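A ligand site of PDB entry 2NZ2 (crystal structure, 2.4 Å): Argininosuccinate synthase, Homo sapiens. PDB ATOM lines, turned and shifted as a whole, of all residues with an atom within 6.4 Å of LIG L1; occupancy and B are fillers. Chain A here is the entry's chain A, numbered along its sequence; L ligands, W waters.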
ATOM      1  N   TYR A  88     -20.968  12.690  24.126  1.00  0.00           N
ATOM      2  CA  TYR A  88     -19.870  12.183  23.300  1.00  0.00           C
ATOM      3  C   TYR A  88     -19.645  13.002  22.030  1.00  0.00           C
ATOM      4  O   TYR A  88     -20.528  13.133  21.197  1.00  0.00           O
ATOM      5  CB  TYR A  88     -20.138  10.705  22.949  1.00  0.00           C
ATOM      6  CG  TYR A  88     -19.033  10.018  22.176  1.00  0.00           C
ATOM      7  CD1 TYR A  88     -17.690  10.171  22.536  1.00  0.00           C
ATOM      8  CD2 TYR A  88     -19.344   9.182  21.089  1.00  0.00           C
ATOM      9  CE1 TYR A  88     -16.687   9.518  21.815  1.00  0.00           C
ATOM     10  CE2 TYR A  88     -18.333   8.533  20.374  1.00  0.00           C
ATOM     11  CZ  TYR A  88     -17.019   8.716  20.741  1.00  0.00           C
ATOM     12  OH  TYR A  88     -16.035   8.083  20.055  1.00  0.00           O
ATOM     13  N   LEU A  90     -17.638  12.226  19.633  1.00  0.00           N
ATOM     14  CA  LEU A  90     -17.532  11.358  18.448  1.00  0.00           C
ATOM     15  C   LEU A  90     -16.126  11.125  17.882  1.00  0.00           C
ATOM     16  O   LEU A  90     -16.001  10.689  16.738  1.00  0.00           O
ATOM     17  CB  LEU A  90     -18.461  11.843  17.326  1.00  0.00           C
ATOM     18  CG  LEU A  90     -19.980  11.907  17.581  1.00  0.00           C
ATOM     19  CD1 LEU A  90     -20.653  12.865  16.560  1.00  0.00           C
ATOM     20  CD2 LEU A  90     -20.626  10.530  17.577  1.00  0.00           C
ATOM     21  N   GLY A  91     -15.084  11.346  18.671  1.00  0.00           N
ATOM     22  CA  GLY A  91     -13.701  11.312  18.186  1.00  0.00           C
ATOM     23  C   GLY A  91     -13.303  10.112  17.347  1.00  0.00           C
ATOM     24  O   GLY A  91     -12.787  10.282  16.254  1.00  0.00           O
ATOM     25  N   THR A  92     -13.545   8.912  17.868  1.00  0.00           N
ATOM     26  CA  THR A  92     -13.285   7.629  17.185  1.00  0.00           C
ATOM     27  C   THR A  92     -14.323   7.340  16.123  1.00  0.00           C
ATOM     28  O   THR A  92     -14.034   6.730  15.079  1.00  0.00           O
ATOM     29  CB  THR A  92     -13.333   6.464  18.195  1.00  0.00           C
ATOM     30  OG1 THR A  92     -12.152   6.471  18.979  1.00  0.00           O
ATOM     31  CG2 THR A  92     -13.444   5.132  17.479  1.00  0.00           C
ATOM     32  N   SER A  93     -15.557   7.748  16.394  1.00  0.00           N
ATOM     33  CA  SER A  93     -16.649   7.434  15.487  1.00  0.00           C
ATOM     34  C   SER A  93     -16.481   8.140  14.136  1.00  0.00           C
ATOM     35  O   SER A  93     -16.704   7.558  13.095  1.00  0.00           O
ATOM     36  CB  SER A  93     -17.973   7.729  16.177  1.00  0.00           C
ATOM     37  OG  SER A  93     -18.386   9.023  15.822  1.00  0.00           O
ATOM     38  N   ARG A  96     -13.340   6.378  11.726  1.00  0.00           N
ATOM     39  CA  ARG A  96     -13.517   5.091  11.027  1.00  0.00           C
ATOM     40  C   ARG A  96     -13.852   5.198   9.547  1.00  0.00           C
ATOM     41  O   ARG A  96     -13.256   4.462   8.772  1.00  0.00           O
ATOM     42  CB  ARG A  96     -14.491   4.146  11.747  1.00  0.00           C
ATOM     43  CG  ARG A  96     -14.201   3.940  13.245  1.00  0.00           C
ATOM     44  CD  ARG A  96     -12.700   3.723  13.521  1.00  0.00           C
ATOM     45  NE  ARG A  96     -12.400   3.309  14.890  1.00  0.00           N
ATOM     46  CZ  ARG A  96     -11.173   3.054  15.346  1.00  0.00           C
ATOM     47  NH1 ARG A  96     -10.110   3.190  14.554  1.00  0.00           N
ATOM     48  NH2 ARG A  96     -10.982   2.655  16.593  1.00  0.00           N
ATOM     49  N   ASN A 124     -18.587  -1.065  18.357  1.00  0.00           N
ATOM     50  CA  ASN A 124     -19.138  -0.163  17.337  1.00  0.00           C
ATOM     51  C   ASN A 124     -18.286  -0.142  16.100  1.00  0.00           C
ATOM     52  O   ASN A 124     -18.804  -0.052  14.999  1.00  0.00           O
ATOM     53  CB  ASN A 124     -19.195   1.254  17.876  1.00  0.00           C
ATOM     54  CG  ASN A 124     -20.282   1.440  18.886  1.00  0.00           C
ATOM     55  OD1 ASN A 124     -21.377   0.879  18.741  1.00  0.00           O
ATOM     56  ND2 ASN A 124     -19.999   2.241  19.905  1.00  0.00           N
ATOM     57  N   ASP A 125     -16.967  -0.215  16.278  1.00  0.00           N
ATOM     58  CA  ASP A 125     -16.030  -0.010  15.155  1.00  0.00           C
ATOM     59  C   ASP A 125     -16.136  -1.063  14.063  1.00  0.00           C
ATOM     60  O   ASP A 125     -15.942  -0.734  12.881  1.00  0.00           O
ATOM     61  CB  ASP A 125     -14.580   0.084  15.640  1.00  0.00           C
ATOM     62  CG  ASP A 125     -14.293   1.360  16.439  1.00  0.00           C
ATOM     63  OD1 ASP A 125     -14.890   2.426  16.176  1.00  0.00           O
ATOM     64  OD2 ASP A 125     -13.417   1.295  17.320  1.00  0.00           O
ATOM     65  N   ARG A 128     -18.702   0.201  11.827  1.00  0.00           N
ATOM     66  CA  ARG A 128     -18.353   1.421  11.117  1.00  0.00           C
ATOM     67  C   ARG A 128     -17.462   1.134   9.912  1.00  0.00           C
ATOM     68  O   ARG A 128     -17.738   1.605   8.817  1.00  0.00           O
ATOM     69  CB  ARG A 128     -17.731   2.469  12.070  1.00  0.00           C
ATOM     70  CG  ARG A 128     -18.626   2.777  13.270  1.00  0.00           C
ATOM     71  CD  ARG A 128     -17.863   3.547  14.366  1.00  0.00           C
ATOM     72  NE  ARG A 128     -18.743   4.096  15.402  1.00  0.00           N
ATOM     73  CZ  ARG A 128     -18.357   4.404  16.626  1.00  0.00           C
ATOM     74  NH1 ARG A 128     -17.098   4.227  17.021  1.00  0.00           N
ATOM     75  NH2 ARG A 128     -19.219   4.877  17.480  1.00  0.00           N
ATOM     76  N   SER A 181      -7.918  -0.670  27.240  1.00  0.00           N
ATOM     77  CA  SER A 181      -7.556  -0.412  25.845  1.00  0.00           C
ATOM     78  C   SER A 181      -7.715   1.078  25.512  1.00  0.00           C
ATOM     79  O   SER A 181      -8.574   1.751  26.080  1.00  0.00           O
ATOM     80  CB  SER A 181      -8.393  -1.277  24.875  1.00  0.00           C
ATOM     81  OG  SER A 181      -9.763  -1.247  25.205  1.00  0.00           O
ATOM     82  N   MET A 182      -6.875   1.553  24.592  1.00  0.00           N
ATOM     83  CA  MET A 182      -6.859   2.962  24.145  1.00  0.00           C
ATOM     84  C   MET A 182      -7.219   3.069  22.663  1.00  0.00           C
ATOM     85  O   MET A 182      -6.864   2.210  21.853  1.00  0.00           O
ATOM     86  CB  MET A 182      -5.499   3.640  24.435  1.00  0.00           C
ATOM     87  CG  MET A 182      -5.189   3.892  25.961  1.00  0.00           C
ATOM     88  SD  MET A 182      -3.493   4.238  26.662  1.00  0.00           S
ATOM     89  CE  MET A 182      -3.172   5.942  26.173  1.00  0.00           C
ATOM     90  N   ASP A 183      -7.968   4.116  22.302  1.00  0.00           N
ATOM     91  CA  ASP A 183      -8.045   4.533  20.907  1.00  0.00           C
ATOM     92  C   ASP A 183      -7.669   5.996  20.785  1.00  0.00           C
ATOM     93  O   ASP A 183      -8.285   6.859  21.391  1.00  0.00           O
ATOM     94  CB  ASP A 183      -9.444   4.290  20.316  1.00  0.00           C
ATOM     95  CG  ASP A 183      -9.460   4.398  18.805  1.00  0.00           C
ATOM     96  OD1 ASP A 183      -8.862   3.523  18.159  1.00  0.00           O
ATOM     97  OD2 ASP A 183     -10.058   5.339  18.268  1.00  0.00           O
ATOM     98  N   HIS A 188      -9.025  12.950  19.632  1.00  0.00           N
ATOM     99  CA  HIS A 188      -9.217  12.539  21.005  1.00  0.00           C
ATOM    100  C   HIS A 188      -8.378  11.342  21.383  1.00  0.00           C
ATOM    101  O   HIS A 188      -7.648  10.760  20.565  1.00  0.00           O
ATOM    102  CB  HIS A 188     -10.709  12.266  21.235  1.00  0.00           C
ATOM    103  CG  HIS A 188     -11.133  10.850  20.965  1.00  0.00           C
ATOM    104  ND1 HIS A 188     -12.229  10.287  21.573  1.00  0.00           N
ATOM    105  CD2 HIS A 188     -10.610   9.888  20.164  1.00  0.00           C
ATOM    106  CE1 HIS A 188     -12.362   9.034  21.149  1.00  0.00           C
ATOM    107  NE2 HIS A 188     -11.389   8.771  20.312  1.00  0.00           N
ATOM    108  N   SER A 190      -9.529   7.747  23.660  1.00  0.00           N
ATOM    109  CA  SER A 190     -10.540   7.004  24.392  1.00  0.00           C
ATOM    110  C   SER A 190      -9.947   5.815  25.170  1.00  0.00           C
ATOM    111  O   SER A 190      -9.087   5.099  24.672  1.00  0.00           O
ATOM    112  CB  SER A 190     -11.607   6.491  23.418  1.00  0.00           C
ATOM    113  OG  SER A 190     -12.259   5.382  23.967  1.00  0.00           O
ATOM    114  N   TYR A 191     -10.386   5.587  26.359  1.00  0.00           N
ATOM    115  CA  TYR A 191      -9.967   4.477  27.128  1.00  0.00           C
ATOM    116  C   TYR A 191     -11.185   3.707  27.577  1.00  0.00           C
ATOM    117  O   TYR A 191     -12.089   4.260  28.068  1.00  0.00           O
ATOM    118  CB  TYR A 191      -9.166   4.980  28.346  1.00  0.00           C
ATOM    119  CG  TYR A 191      -8.165   6.091  28.144  1.00  0.00           C
ATOM    120  CD1 TYR A 191      -8.560   7.391  28.024  1.00  0.00           C
ATOM    121  CD2 TYR A 191      -6.846   5.838  28.123  1.00  0.00           C
ATOM    122  CE1 TYR A 191      -7.682   8.364  27.876  1.00  0.00           C
ATOM    123  CE2 TYR A 191      -5.964   6.802  27.974  1.00  0.00           C
ATOM    124  CZ  TYR A 191      -6.355   8.080  27.860  1.00  0.00           C
ATOM    125  OH  TYR A 191      -5.416   9.004  27.703  1.00  0.00           O
ATOM    126  N   GLU A 192     -11.195   2.389  27.434  1.00  0.00           N
ATOM    127  CA  GLU A 192     -12.417   1.593  27.673  1.00  0.00           C
ATOM    128  C   GLU A 192     -12.563   0.240  28.324  1.00  0.00           C
ATOM    129  O   GLU A 192     -13.527  -0.037  28.956  1.00  0.00           O
ATOM    130  CB  GLU A 192     -13.597   1.928  26.820  1.00  0.00           C
ATOM    131  CG  GLU A 192     -13.610   1.241  25.540  1.00  0.00           C
ATOM    132  CD  GLU A 192     -14.791   1.567  24.745  1.00  0.00           C
ATOM    133  OE1 GLU A 192     -15.127   2.713  24.721  1.00  0.00           O
ATOM    134  OE2 GLU A 192     -15.412   0.692  24.185  1.00  0.00           O
ATOM    135  N   ALA A 193     -11.599  -0.690  28.096  1.00  0.00           N
ATOM    136  CA  ALA A 193     -11.905  -1.922  28.789  1.00  0.00           C
ATOM    137  C   ALA A 193     -11.224  -2.076  30.134  1.00  0.00           C
ATOM    138  O   ALA A 193     -10.949  -1.136  30.786  1.00  0.00           O
ATOM    139  CB  ALA A 193     -11.673  -3.019  27.955  1.00  0.00           C
ATOM    140  N   GLU A 271     -22.234   4.954  27.713  1.00  0.00           N
ATOM    141  CA  GLU A 271     -22.856   5.130  26.400  1.00  0.00           C
ATOM    142  C   GLU A 271     -23.516   3.833  25.890  1.00  0.00           C
ATOM    143  O   GLU A 271     -23.182   2.716  26.308  1.00  0.00           O
ATOM    144  CB  GLU A 271     -21.793   5.559  25.408  1.00  0.00           C
ATOM    145  CG  GLU A 271     -20.896   4.424  24.944  1.00  0.00           C
ATOM    146  CD  GLU A 271     -19.640   4.916  24.255  1.00  0.00           C
ATOM    147  OE1 GLU A 271     -18.754   5.481  24.944  1.00  0.00           O
ATOM    148  OE2 GLU A 271     -19.521   4.686  23.044  1.00  0.00           O
ATOM    149  N   ARG A 273     -24.516   1.237  22.586  1.00  0.00           N
ATOM    150  CA  ARG A 273     -23.394   0.875  21.748  1.00  0.00           C
ATOM    151  C   ARG A 273     -24.456   0.546  20.668  1.00  0.00           C
ATOM    152  O   ARG A 273     -25.648   0.366  21.006  1.00  0.00           O
ATOM    153  CB  ARG A 273     -22.649  -0.400  22.149  1.00  0.00           C
ATOM    154  CG  ARG A 273     -21.235  -0.142  22.607  1.00  0.00           C
ATOM    155  CD  ARG A 273     -20.401  -1.421  22.627  1.00  0.00           C
ATOM    156  NE  ARG A 273     -19.088  -1.124  23.189  1.00  0.00           N
ATOM    157  CZ  ARG A 273     -18.264  -2.009  23.725  1.00  0.00           C
ATOM    158  NH1 ARG A 273     -18.581  -3.284  23.787  1.00  0.00           N
ATOM    159  NH2 ARG A 273     -17.103  -1.595  24.231  1.00  0.00           N
ATOM    160  N   SER A 279     -21.806   0.697  27.496  1.00  0.00           N
ATOM    161  CA  SER A 279     -20.366   0.629  27.699  1.00  0.00           C
ATOM    162  C   SER A 279     -19.854   1.847  28.447  1.00  0.00           C
ATOM    163  O   SER A 279     -20.372   2.946  28.270  1.00  0.00           O
ATOM    164  CB  SER A 279     -19.656   0.450  26.344  1.00  0.00           C
ATOM    165  OG  SER A 279     -18.257   0.424  26.515  1.00  0.00           O
ATOM    166  N   GLY A 281     -16.816   4.525  29.170  1.00  0.00           N
ATOM    167  CA  GLY A 281     -15.704   5.111  28.458  1.00  0.00           C
ATOM    168  C   GLY A 281     -15.348   6.461  29.043  1.00  0.00           C
ATOM    169  O   GLY A 281     -16.225   7.247  29.462  1.00  0.00           O
ATOM    170  N   TYR A 283     -12.984   9.901  27.911  1.00  0.00           N
ATOM    171  CA  TYR A 283     -12.510  10.522  26.707  1.00  0.00           C
ATOM    172  C   TYR A 283     -11.731  11.782  27.002  1.00  0.00           C
ATOM    173  O   TYR A 283     -11.969  12.466  27.995  1.00  0.00           O
ATOM    174  CB  TYR A 283     -13.680  10.818  25.771  1.00  0.00           C
ATOM    175  CG  TYR A 283     -14.455   9.596  25.384  1.00  0.00           C
ATOM    176  CD1 TYR A 283     -14.061   8.816  24.308  1.00  0.00           C
ATOM    177  CD2 TYR A 283     -15.579   9.203  26.094  1.00  0.00           C
ATOM    178  CE1 TYR A 283     -14.774   7.661  23.948  1.00  0.00           C
ATOM    179  CE2 TYR A 283     -16.306   8.063  25.745  1.00  0.00           C
ATOM    180  CZ  TYR A 283     -15.888   7.304  24.680  1.00  0.00           C
ATOM    181  OH  TYR A 283     -16.587   6.183  24.354  1.00  0.00           O
ATOM    182  N   TYR A 323     -22.218   7.884  14.925  1.00  0.00           N
ATOM    183  CA  TYR A 323     -21.939   6.922  15.993  1.00  0.00           C
ATOM    184  C   TYR A 323     -22.189   5.470  15.590  1.00  0.00           C
ATOM    185  O   TYR A 323     -21.372   4.569  15.916  1.00  0.00           O
ATOM    186  CB  TYR A 323     -22.697   7.244  17.280  1.00  0.00           C
ATOM    187  CG  TYR A 323     -22.354   6.318  18.438  1.00  0.00           C
ATOM    188  CD1 TYR A 323     -21.235   6.549  19.240  1.00  0.00           C
ATOM    189  CD2 TYR A 323     -23.159   5.200  18.743  1.00  0.00           C
ATOM    190  CE1 TYR A 323     -20.926   5.714  20.279  1.00  0.00           C
ATOM    191  CE2 TYR A 323     -22.852   4.361  19.804  1.00  0.00           C
ATOM    192  CZ  TYR A 323     -21.733   4.630  20.573  1.00  0.00           C
ATOM    193  OH  TYR A 323     -21.408   3.780  21.615  1.00  0.00           O
HETATM  194  C1  LIG L   1     -16.948   4.767  20.277  1.00  0.00           C
HETATM  195  O1  LIG L   1     -17.718   3.804  20.098  1.00  0.00           O
HETATM  196  O2  LIG L   1     -16.695   5.567  19.362  1.00  0.00           O
HETATM  197  C2  LIG L   1     -16.348   4.928  21.642  1.00  0.00           C
HETATM  198  N1  LIG L   1     -17.102   4.083  22.560  1.00  0.00           N
HETATM  199  C3  LIG L   1     -14.886   4.494  21.632  1.00  0.00           C
HETATM  200  C4  LIG L   1     -14.679   3.064  21.104  1.00  0.00           C
HETATM  201  C5  LIG L   1     -13.265   2.891  20.605  1.00  0.00           C
HETATM  202  N2  LIG L   1     -12.313   3.084  21.687  1.00  0.00           N
HETATM  203  C6  LIG L   1     -11.538   2.089  22.147  1.00  0.00           C
HETATM  204  O3  LIG L   1     -11.500   0.991  21.630  1.00  0.00           O
HETATM  205  N3  LIG L   1     -10.792   2.325  23.210  1.00  0.00           N
HETATM  206  N1  LG2 L   2     -12.849  -0.564  19.413  1.00  0.00           N
HETATM  207  C1  LG2 L   2     -13.478  -1.352  20.467  1.00  0.00           C
HETATM  208  C2  LG2 L   2     -13.842  -2.751  19.968  1.00  0.00           C
HETATM  209  O1  LG2 L   2     -14.459  -3.528  20.687  1.00  0.00           O
HETATM  210  C3  LG2 L   2     -14.715  -0.644  21.009  1.00  0.00           C
HETATM  211  C4  LG2 L   2     -15.733  -0.346  19.917  1.00  0.00           C
HETATM  212  O2  LG2 L   2     -16.729   0.340  20.211  1.00  0.00           O
HETATM  213  O3  LG2 L   2     -15.535  -0.817  18.777  1.00  0.00           O
HETATM  214  O4  LG2 L   2     -13.460  -3.146  18.858  1.00  0.00           O
HETATM  215  O   HOH W   1      -9.434   0.017  19.854  1.00  0.00           O
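The side-chain carboxylate (OE2) of Glu 271 lies within salt-bridge range of a nitrogen (N1) of LIG L1, 2.5 Å away.
The side-chain hydroxyl of Tyr 88 sits at hydrogen-bond distance from an oxygen (O2) of LIG L1, 2.7 Å away.
NH1 of Arg 128 is in salt-bridge range of O2 of LIG L1 (2.7 Å).
ND2 of Asn 124 lies within hydrogen-bond range of O1 of LIG L1, 2.8 Å away.
The side-chain hydroxyl (OH) of Tyr 283 sits at hydrogen-bond distance from a nitrogen (N1) of LIG L1 (2.8 Å).
OE1 of Glu 192 lies within salt-bridge range of N1 of LIG L1 (3.2 Å).
N2 of LIG L1 sits at hydrogen-bond distance from OG of Ser 190 (3.2 Å).
An oxygen (O2) of LG2 L2 sits at hydrogen-bond distance from the backbone NH (N) of Asn 124 (3.0 Å).
O3 of LG2 L2 sits at hydrogen-bond distance from N of Asp 125 (2.9 Å).
N1 of LG2 L2 is in salt-bridge range of OD2 of Asp 125 (2.9 Å).
A nitrogen (N1) of LG2 L2 lies within hydrogen-bond range of an oxygen (O3) of LIG L1, at 3.0 Å.
O of Glu 271 sits at hydrogen-bond distance from N of Ser 279 (2.7 Å).
The backbone NH (N) of Thr 92 sits at hydrogen-bond distance from the side-chain hydroxyl (OH) of Tyr 88, at 3.4 Å.
NH1 of Arg 128 is in salt-bridge range of OD1 of Asp 125 (3.0 Å).
The backbone NH of Glu 192 sits at hydrogen-bond distance from the backbone carbonyl oxygen of Ser 181.
The side-chain hydroxyl (OG1) of Thr 92 lies within hydrogen-bond range of the side-chain carboxylate (OD2) of Asp 183 (2.5 Å).
The guanidinium group of Arg 96 is in salt-bridge range of the side-chain carboxylate of Asp 183 (2.8 Å).
A ring nitrogen (NE2) of His 188 sits at hydrogen-bond distance from the side-chain hydroxyl (OG1) of Thr 92, 2.8 Å away.
The side-chain hydroxyl (OG) of Ser 181 sits at hydrogen-bond distance from the backbone NH (N) of Ala 193.
The backbone NH (N) of Asp 183 sits close to a nitrogen (N3) of LIG L1.
Residues that only touch LIG L1: Thr 92 (3.7 Å), Ser 93 (3.9 Å), Asp 125 (3.7 Å), Ser 181 (3.7 Å), Met 182 (3.7 Å) and Tyr 323 (3.7 Å).
Hydrophobic or aromatic side chains that line LIG L1: Tyr 88, Tyr 283 and Tyr 323.
Water W1 lies within hydrogen-bond range of O3 of LIG L1 (2.9 Å) and N1 of LG2 L2 (3.5 Å).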
